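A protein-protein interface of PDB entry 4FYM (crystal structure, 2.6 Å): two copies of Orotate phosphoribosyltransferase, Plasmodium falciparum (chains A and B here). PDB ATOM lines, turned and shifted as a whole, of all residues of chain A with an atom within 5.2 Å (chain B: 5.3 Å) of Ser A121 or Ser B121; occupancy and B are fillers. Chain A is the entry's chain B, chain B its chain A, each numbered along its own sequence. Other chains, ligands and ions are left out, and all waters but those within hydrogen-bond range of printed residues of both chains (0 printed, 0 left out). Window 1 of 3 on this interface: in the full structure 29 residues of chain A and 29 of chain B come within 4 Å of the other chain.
The backbone carbonyl oxygen (O) of Pro B118 is in hydrogen-bond range of the side-chain hydroxyl (OG) of Ser A121.
The side-chain hydroxyl of Ser B121 is in hydrogen-bond range of the backbone carbonyl oxygen of Pro A118, at 2.9 Å.
OG of Ser A121 lies within hydrogen-bond range of OG of Ser B121 (2.8 Å).
O of Pro B118 sits at hydrogen-bond distance from OG of Ser B121 (3.4 Å).
O of Pro A118 is in hydrogen-bond range of OG of Ser A121, 3.4 Å away.
Among the printed residues, merely in contact across the chains: His A125 with His B125 (3.4 Å), Ile A117 with Ile B117 (3.7 Å), Ile A117 with Pro B118 (3.8 Å), Pro A118 with Ile B117 (3.8 Å), His A125 with Ile B85 (3.8 Å), Ile A85 with His B125 (3.8 Å), Ile A85 with Tyr B138 (3.9 Å), Tyr A138 with Ile B85 (3.9 Å), Ser A121 with Ile B85 (3.9 Å) and Ile A85 with Ser B121 (3.97 Å).
Of chain B, only Ile B85, Pro B118 and Ser B121 come within 4 Å of Ser A121.
Ser B121 touches just these residues of chain A: Ile A85, Pro A118 and Ser A121.
Printed residues of chain B within 4 Å of Ile A117: Ile B117 (3.7 Å) and Pro B118 (3.8 Å).
Of the printed residues of chain A, Ile B117 touches Ile A117 and Pro A118.
Of the printed residues of chain B, Pro A118 touches Ile B117 and Ser B121.
Leu A122 touches none of the printed residues of chain B.
The nearest printed residue of chain B that does not touch Pro A118 is Tyr B138 (4.05 Å).
Hydrophobic or aromatic side chains of chain A that line the printed part of chain B: Ile A85, Ile A117, Pro A118, His A125 and Tyr A138.
Hydrophobic or aromatic side chains of chain B within 4 Å of the printed part of chain A: Ile B85, Ile B117, Pro B118, His B125 and Tyr B138.
Among the printed residues, 13 pairs touch across the chains.
Among the printed residues, no Asp or Glu carboxylate lies within 4 Å of a Lys or Arg side-chain nitrogen of the other chain.
Ile A85 touches His B125, and with the chains exchanged His A125 touches Ile B85.
Ile A117 touches Pro B118, and with the chains exchanged Pro A118 touches Ile B117.
Ser B121 touches its own counterpart, Ser A121.
His A125 touches its own counterpart, His B125.
Positions printed for both chains: 85, 117, 118, 119, 120, 121, 122, 123, 124, 125 and 138.
Of the 13 pairs that touch across the chains among the printed residues, 13 have their exchanged pair printed and touching as well.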
ATOM      1  N   ILE A  85       5.467 -20.440 -16.399  1.00  0.00           N
ATOM      2  CA  ILE A  85       4.393 -20.217 -17.353  1.00  0.00           C
ATOM      3  C   ILE A  85       3.787 -18.824 -17.237  1.00  0.00           C
ATOM      4  O   ILE A  85       3.415 -18.239 -18.264  1.00  0.00           O
ATOM      5  CB  ILE A  85       3.310 -21.321 -17.232  1.00  0.00           C
ATOM      6  CG1 ILE A  85       2.353 -21.309 -18.430  1.00  0.00           C
ATOM      7  CG2 ILE A  85       2.482 -21.128 -16.015  1.00  0.00           C
ATOM      8  CD1 ILE A  85       3.008 -21.689 -19.766  1.00  0.00           C
ATOM      9  N   ILE A 117      13.919 -22.698 -27.288  1.00  0.00           N
ATOM     10  CA  ILE A 117      13.222 -23.915 -27.529  1.00  0.00           C
ATOM     11  C   ILE A 117      11.901 -23.983 -26.758  1.00  0.00           C
ATOM     12  O   ILE A 117      10.882 -24.286 -27.334  1.00  0.00           O
ATOM     13  CB  ILE A 117      14.113 -25.143 -27.310  1.00  0.00           C
ATOM     14  CG1 ILE A 117      15.332 -25.038 -28.230  1.00  0.00           C
ATOM     15  CG2 ILE A 117      13.360 -26.450 -27.617  1.00  0.00           C
ATOM     16  CD1 ILE A 117      16.298 -26.214 -28.164  1.00  0.00           C
ATOM     17  N   PRO A 118      11.901 -23.716 -25.465  1.00  0.00           N
ATOM     18  CA  PRO A 118      10.602 -23.722 -24.778  1.00  0.00           C
ATOM     19  C   PRO A 118       9.723 -22.580 -25.179  1.00  0.00           C
ATOM     20  O   PRO A 118       8.483 -22.732 -25.194  1.00  0.00           O
ATOM     21  CB  PRO A 118      10.955 -23.635 -23.301  1.00  0.00           C
ATOM     22  CG  PRO A 118      12.312 -23.022 -23.269  1.00  0.00           C
ATOM     23  CD  PRO A 118      13.007 -23.353 -24.564  1.00  0.00           C
ATOM     24  N   MET A 119      10.345 -21.496 -25.646  1.00  0.00           N
ATOM     25  CA  MET A 119       9.561 -20.413 -26.270  1.00  0.00           C
ATOM     26  C   MET A 119       8.829 -20.756 -27.596  1.00  0.00           C
ATOM     27  O   MET A 119       7.732 -20.230 -27.878  1.00  0.00           O
ATOM     28  CB  MET A 119      10.446 -19.193 -26.490  1.00  0.00           C
ATOM     29  CG  MET A 119      10.799 -18.506 -25.158  1.00  0.00           C
ATOM     30  SD  MET A 119      12.031 -17.211 -25.362  1.00  0.00           S
ATOM     31  CE  MET A 119      11.314 -16.063 -26.455  1.00  0.00           C
ATOM     32  N   VAL A 120       9.397 -21.645 -28.391  1.00  0.00           N
ATOM     33  CA  VAL A 120       8.866 -21.797 -29.714  1.00  0.00           C
ATOM     34  C   VAL A 120       7.553 -22.553 -29.713  1.00  0.00           C
ATOM     35  O   VAL A 120       6.627 -22.240 -30.502  1.00  0.00           O
ATOM     36  CB  VAL A 120       9.895 -22.422 -30.666  1.00  0.00           C
ATOM     37  CG1 VAL A 120      10.040 -23.942 -30.470  1.00  0.00           C
ATOM     38  CG2 VAL A 120       9.482 -22.174 -32.108  1.00  0.00           C
ATOM     39  N   SER A 121       7.437 -23.564 -28.857  1.00  0.00           N
ATOM     40  CA  SER A 121       6.148 -24.303 -28.775  1.00  0.00           C
ATOM     41  C   SER A 121       5.065 -23.419 -28.238  1.00  0.00           C
ATOM     42  O   SER A 121       3.963 -23.363 -28.753  1.00  0.00           O
ATOM     43  CB  SER A 121       6.267 -25.562 -27.921  1.00  0.00           C
ATOM     44  OG  SER A 121       6.718 -25.228 -26.657  1.00  0.00           O
ATOM     45  N   LEU A 122       5.371 -22.676 -27.220  1.00  0.00           N
ATOM     46  CA  LEU A 122       4.339 -21.875 -26.574  1.00  0.00           C
ATOM     47  C   LEU A 122       3.968 -20.696 -27.486  1.00  0.00           C
ATOM     48  O   LEU A 122       2.817 -20.295 -27.560  1.00  0.00           O
ATOM     49  CB  LEU A 122       4.867 -21.406 -25.230  1.00  0.00           C
ATOM     50  CG  LEU A 122       3.875 -20.785 -24.314  1.00  0.00           C
ATOM     51  CD1 LEU A 122       2.735 -21.750 -23.977  1.00  0.00           C
ATOM     52  CD2 LEU A 122       4.603 -20.408 -23.067  1.00  0.00           C
ATOM     53  N   THR A 123       4.933 -20.110 -28.185  1.00  0.00           N
ATOM     54  CA  THR A 123       4.606 -19.054 -29.146  1.00  0.00           C
ATOM     55  C   THR A 123       3.715 -19.619 -30.229  1.00  0.00           C
ATOM     56  O   THR A 123       2.730 -18.990 -30.670  1.00  0.00           O
ATOM     57  CB  THR A 123       5.880 -18.511 -29.783  1.00  0.00           C
ATOM     58  OG1 THR A 123       6.694 -17.911 -28.754  1.00  0.00           O
ATOM     59  CG2 THR A 123       5.538 -17.503 -30.831  1.00  0.00           C
ATOM     60  N   SER A 124       4.033 -20.830 -30.661  1.00  0.00           N
ATOM     61  CA  SER A 124       3.181 -21.524 -31.637  1.00  0.00           C
ATOM     62  C   SER A 124       1.793 -21.661 -31.135  1.00  0.00           C
ATOM     63  O   SER A 124       0.816 -21.469 -31.867  1.00  0.00           O
ATOM     64  CB  SER A 124       3.776 -22.905 -32.001  1.00  0.00           C
ATOM     65  OG  SER A 124       5.008 -22.714 -32.721  1.00  0.00           O
ATOM     66  N   HIS A 125       1.665 -21.988 -29.871  1.00  0.00           N
ATOM     67  CA  HIS A 125       0.319 -22.061 -29.285  1.00  0.00           C
ATOM     68  C   HIS A 125      -0.419 -20.734 -29.388  1.00  0.00           C
ATOM     69  O   HIS A 125      -1.576 -20.707 -29.754  1.00  0.00           O
ATOM     70  CB  HIS A 125       0.444 -22.462 -27.827  1.00  0.00           C
ATOM     71  CG  HIS A 125      -0.716 -22.079 -27.008  1.00  0.00           C
ATOM     72  ND1 HIS A 125      -1.857 -22.843 -26.945  1.00  0.00           N
ATOM     73  CD2 HIS A 125      -0.933 -21.015 -26.222  1.00  0.00           C
ATOM     74  CE1 HIS A 125      -2.729 -22.271 -26.150  1.00  0.00           C
ATOM     75  NE2 HIS A 125      -2.182 -21.164 -25.688  1.00  0.00           N
ATOM     76  N   TYR A 138       7.189 -26.211 -35.891  1.00  0.00           N
ATOM     77  CA  TYR A 138       8.355 -25.583 -35.302  1.00  0.00           C
ATOM     78  C   TYR A 138       9.599 -26.495 -35.337  1.00  0.00           C
ATOM     79  O   TYR A 138       9.489 -27.693 -35.457  1.00  0.00           O
ATOM     80  CB  TYR A 138       8.069 -25.062 -33.928  1.00  0.00           C
ATOM     81  CG  TYR A 138       7.391 -26.008 -32.982  1.00  0.00           C
ATOM     82  CD1 TYR A 138       8.115 -26.895 -32.255  1.00  0.00           C
ATOM     83  CD2 TYR A 138       5.997 -25.992 -32.797  1.00  0.00           C
ATOM     84  CE1 TYR A 138       7.496 -27.762 -31.362  1.00  0.00           C
ATOM     85  CE2 TYR A 138       5.374 -26.874 -31.924  1.00  0.00           C
ATOM     86  CZ  TYR A 138       6.131 -27.739 -31.190  1.00  0.00           C
ATOM     87  OH  TYR A 138       5.555 -28.558 -30.228  1.00  0.00           O
ATOM     88  N   ILE B  85       1.979 -27.957 -33.590  1.00  0.00           N
ATOM     89  CA  ILE B  85       1.164 -27.658 -32.438  1.00  0.00           C
ATOM     90  C   ILE B  85      -0.042 -28.594 -32.378  1.00  0.00           C
ATOM     91  O   ILE B  85      -0.507 -28.935 -31.308  1.00  0.00           O
ATOM     92  CB  ILE B  85       0.775 -26.171 -32.430  1.00  0.00           C
ATOM     93  CG1 ILE B  85       0.145 -25.728 -31.129  1.00  0.00           C
ATOM     94  CG2 ILE B  85      -0.215 -25.888 -33.512  1.00  0.00           C
ATOM     95  CD1 ILE B  85       1.059 -25.765 -29.909  1.00  0.00           C
ATOM     96  N   ILE B 117      12.099 -30.590 -24.196  1.00  0.00           N
ATOM     97  CA  ILE B 117      12.115 -29.193 -23.936  1.00  0.00           C
ATOM     98  C   ILE B 117      10.902 -28.466 -24.517  1.00  0.00           C
ATOM     99  O   ILE B 117      10.256 -27.715 -23.814  1.00  0.00           O
ATOM    100  CB  ILE B 117      13.453 -28.549 -24.383  1.00  0.00           C
ATOM    101  CG1 ILE B 117      14.585 -29.266 -23.671  1.00  0.00           C
ATOM    102  CG2 ILE B 117      13.502 -27.079 -24.024  1.00  0.00           C
ATOM    103  CD1 ILE B 117      15.966 -28.725 -23.939  1.00  0.00           C
ATOM    104  N   PRO B 118      10.585 -28.650 -25.803  1.00  0.00           N
ATOM    105  CA  PRO B 118       9.356 -27.978 -26.271  1.00  0.00           C
ATOM    106  C   PRO B 118       8.094 -28.572 -25.689  1.00  0.00           C
ATOM    107  O   PRO B 118       7.121 -27.829 -25.487  1.00  0.00           O
ATOM    108  CB  PRO B 118       9.380 -28.149 -27.788  1.00  0.00           C
ATOM    109  CG  PRO B 118      10.253 -29.343 -28.004  1.00  0.00           C
ATOM    110  CD  PRO B 118      11.207 -29.466 -26.856  1.00  0.00           C
ATOM    111  N   MET B 119       8.157 -29.831 -25.279  1.00  0.00           N
ATOM    112  CA  MET B 119       7.044 -30.418 -24.491  1.00  0.00           C
ATOM    113  C   MET B 119       6.815 -29.827 -23.084  1.00  0.00           C
ATOM    114  O   MET B 119       5.683 -29.743 -22.609  1.00  0.00           O
ATOM    115  CB  MET B 119       7.251 -31.920 -24.372  1.00  0.00           C
ATOM    116  CG  MET B 119       7.037 -32.653 -25.697  1.00  0.00           C
ATOM    117  SD  MET B 119       7.467 -34.415 -25.610  1.00  0.00           S
ATOM    118  CE  MET B 119       6.447 -35.071 -24.377  1.00  0.00           C
ATOM    119  N   VAL B 120       7.868 -29.372 -22.411  1.00  0.00           N
ATOM    120  CA  VAL B 120       7.701 -29.015 -21.027  1.00  0.00           C
ATOM    121  C   VAL B 120       6.932 -27.708 -20.868  1.00  0.00           C
ATOM    122  O   VAL B 120       6.146 -27.542 -19.928  1.00  0.00           O
ATOM    123  CB  VAL B 120       9.069 -29.019 -20.282  1.00  0.00           C
ATOM    124  CG1 VAL B 120       9.894 -27.775 -20.560  1.00  0.00           C
ATOM    125  CG2 VAL B 120       8.822 -29.102 -18.808  1.00  0.00           C
ATOM    126  N   SER B 121       7.186 -26.748 -21.748  1.00  0.00           N
ATOM    127  CA  SER B 121       6.464 -25.468 -21.640  1.00  0.00           C
ATOM    128  C   SER B 121       5.049 -25.672 -21.968  1.00  0.00           C
ATOM    129  O   SER B 121       4.151 -25.178 -21.286  1.00  0.00           O
ATOM    130  CB  SER B 121       7.060 -24.387 -22.557  1.00  0.00           C
ATOM    131  OG  SER B 121       7.077 -24.846 -23.872  1.00  0.00           O
ATOM    132  N   LEU B 122       4.796 -26.433 -22.997  1.00  0.00           N
ATOM    133  CA  LEU B 122       3.404 -26.613 -23.443  1.00  0.00           C
ATOM    134  C   LEU B 122       2.639 -27.511 -22.421  1.00  0.00           C
ATOM    135  O   LEU B 122       1.476 -27.251 -22.135  1.00  0.00           O
ATOM    136  CB  LEU B 122       3.387 -27.207 -24.800  1.00  0.00           C
ATOM    137  CG  LEU B 122       2.083 -27.201 -25.520  1.00  0.00           C
ATOM    138  CD1 LEU B 122       1.589 -25.783 -25.718  1.00  0.00           C
ATOM    139  CD2 LEU B 122       2.320 -27.856 -26.864  1.00  0.00           C
ATOM    140  N   THR B 123       3.312 -28.502 -21.828  1.00  0.00           N
ATOM    141  CA  THR B 123       2.691 -29.287 -20.801  1.00  0.00           C
ATOM    142  C   THR B 123       2.381 -28.412 -19.577  1.00  0.00           C
ATOM    143  O   THR B 123       1.252 -28.464 -19.005  1.00  0.00           O
ATOM    144  CB  THR B 123       3.593 -30.413 -20.377  1.00  0.00           C
ATOM    145  OG1 THR B 123       3.796 -31.273 -21.474  1.00  0.00           O
ATOM    146  CG2 THR B 123       2.948 -31.187 -19.223  1.00  0.00           C
ATOM    147  N   SER B 124       3.319 -27.544 -19.244  1.00  0.00           N
ATOM    148  CA  SER B 124       3.061 -26.541 -18.222  1.00  0.00           C
ATOM    149  C   SER B 124       1.869 -25.703 -18.517  1.00  0.00           C
ATOM    150  O   SER B 124       1.023 -25.428 -17.631  1.00  0.00           O
ATOM    151  CB  SER B 124       4.287 -25.634 -18.055  1.00  0.00           C
ATOM    152  OG  SER B 124       5.344 -26.401 -17.506  1.00  0.00           O
ATOM    153  N   HIS B 125       1.724 -25.304 -19.767  1.00  0.00           N
ATOM    154  CA  HIS B 125       0.509 -24.563 -20.152  1.00  0.00           C
ATOM    155  C   HIS B 125      -0.793 -25.340 -19.866  1.00  0.00           C
ATOM    156  O   HIS B 125      -1.722 -24.800 -19.307  1.00  0.00           O
ATOM    157  CB  HIS B 125       0.584 -24.160 -21.604  1.00  0.00           C
ATOM    158  CG  HIS B 125      -0.726 -23.873 -22.200  1.00  0.00           C
ATOM    159  ND1 HIS B 125      -1.352 -22.665 -22.060  1.00  0.00           N
ATOM    160  CD2 HIS B 125      -1.568 -24.657 -22.904  1.00  0.00           C
ATOM    161  CE1 HIS B 125      -2.512 -22.704 -22.689  1.00  0.00           C
ATOM    162  NE2 HIS B 125      -2.678 -23.915 -23.178  1.00  0.00           N
ATOM    163  N   TYR B 138       9.450 -24.603 -14.826  1.00  0.00           N
ATOM    164  CA  TYR B 138      10.027 -25.712 -15.585  1.00  0.00           C
ATOM    165  C   TYR B 138      11.501 -25.548 -15.813  1.00  0.00           C
ATOM    166  O   TYR B 138      12.048 -24.432 -15.757  1.00  0.00           O
ATOM    167  CB  TYR B 138       9.280 -25.941 -16.882  1.00  0.00           C
ATOM    168  CG  TYR B 138       9.027 -24.719 -17.732  1.00  0.00           C
ATOM    169  CD1 TYR B 138       9.947 -24.302 -18.633  1.00  0.00           C
ATOM    170  CD2 TYR B 138       7.842 -24.030 -17.676  1.00  0.00           C
ATOM    171  CE1 TYR B 138       9.713 -23.233 -19.470  1.00  0.00           C
ATOM    172  CE2 TYR B 138       7.577 -22.956 -18.535  1.00  0.00           C
ATOM    173  CZ  TYR B 138       8.515 -22.579 -19.433  1.00  0.00           C
ATOM    174  OH  TYR B 138       8.297 -21.497 -20.294  1.00  0.00           O
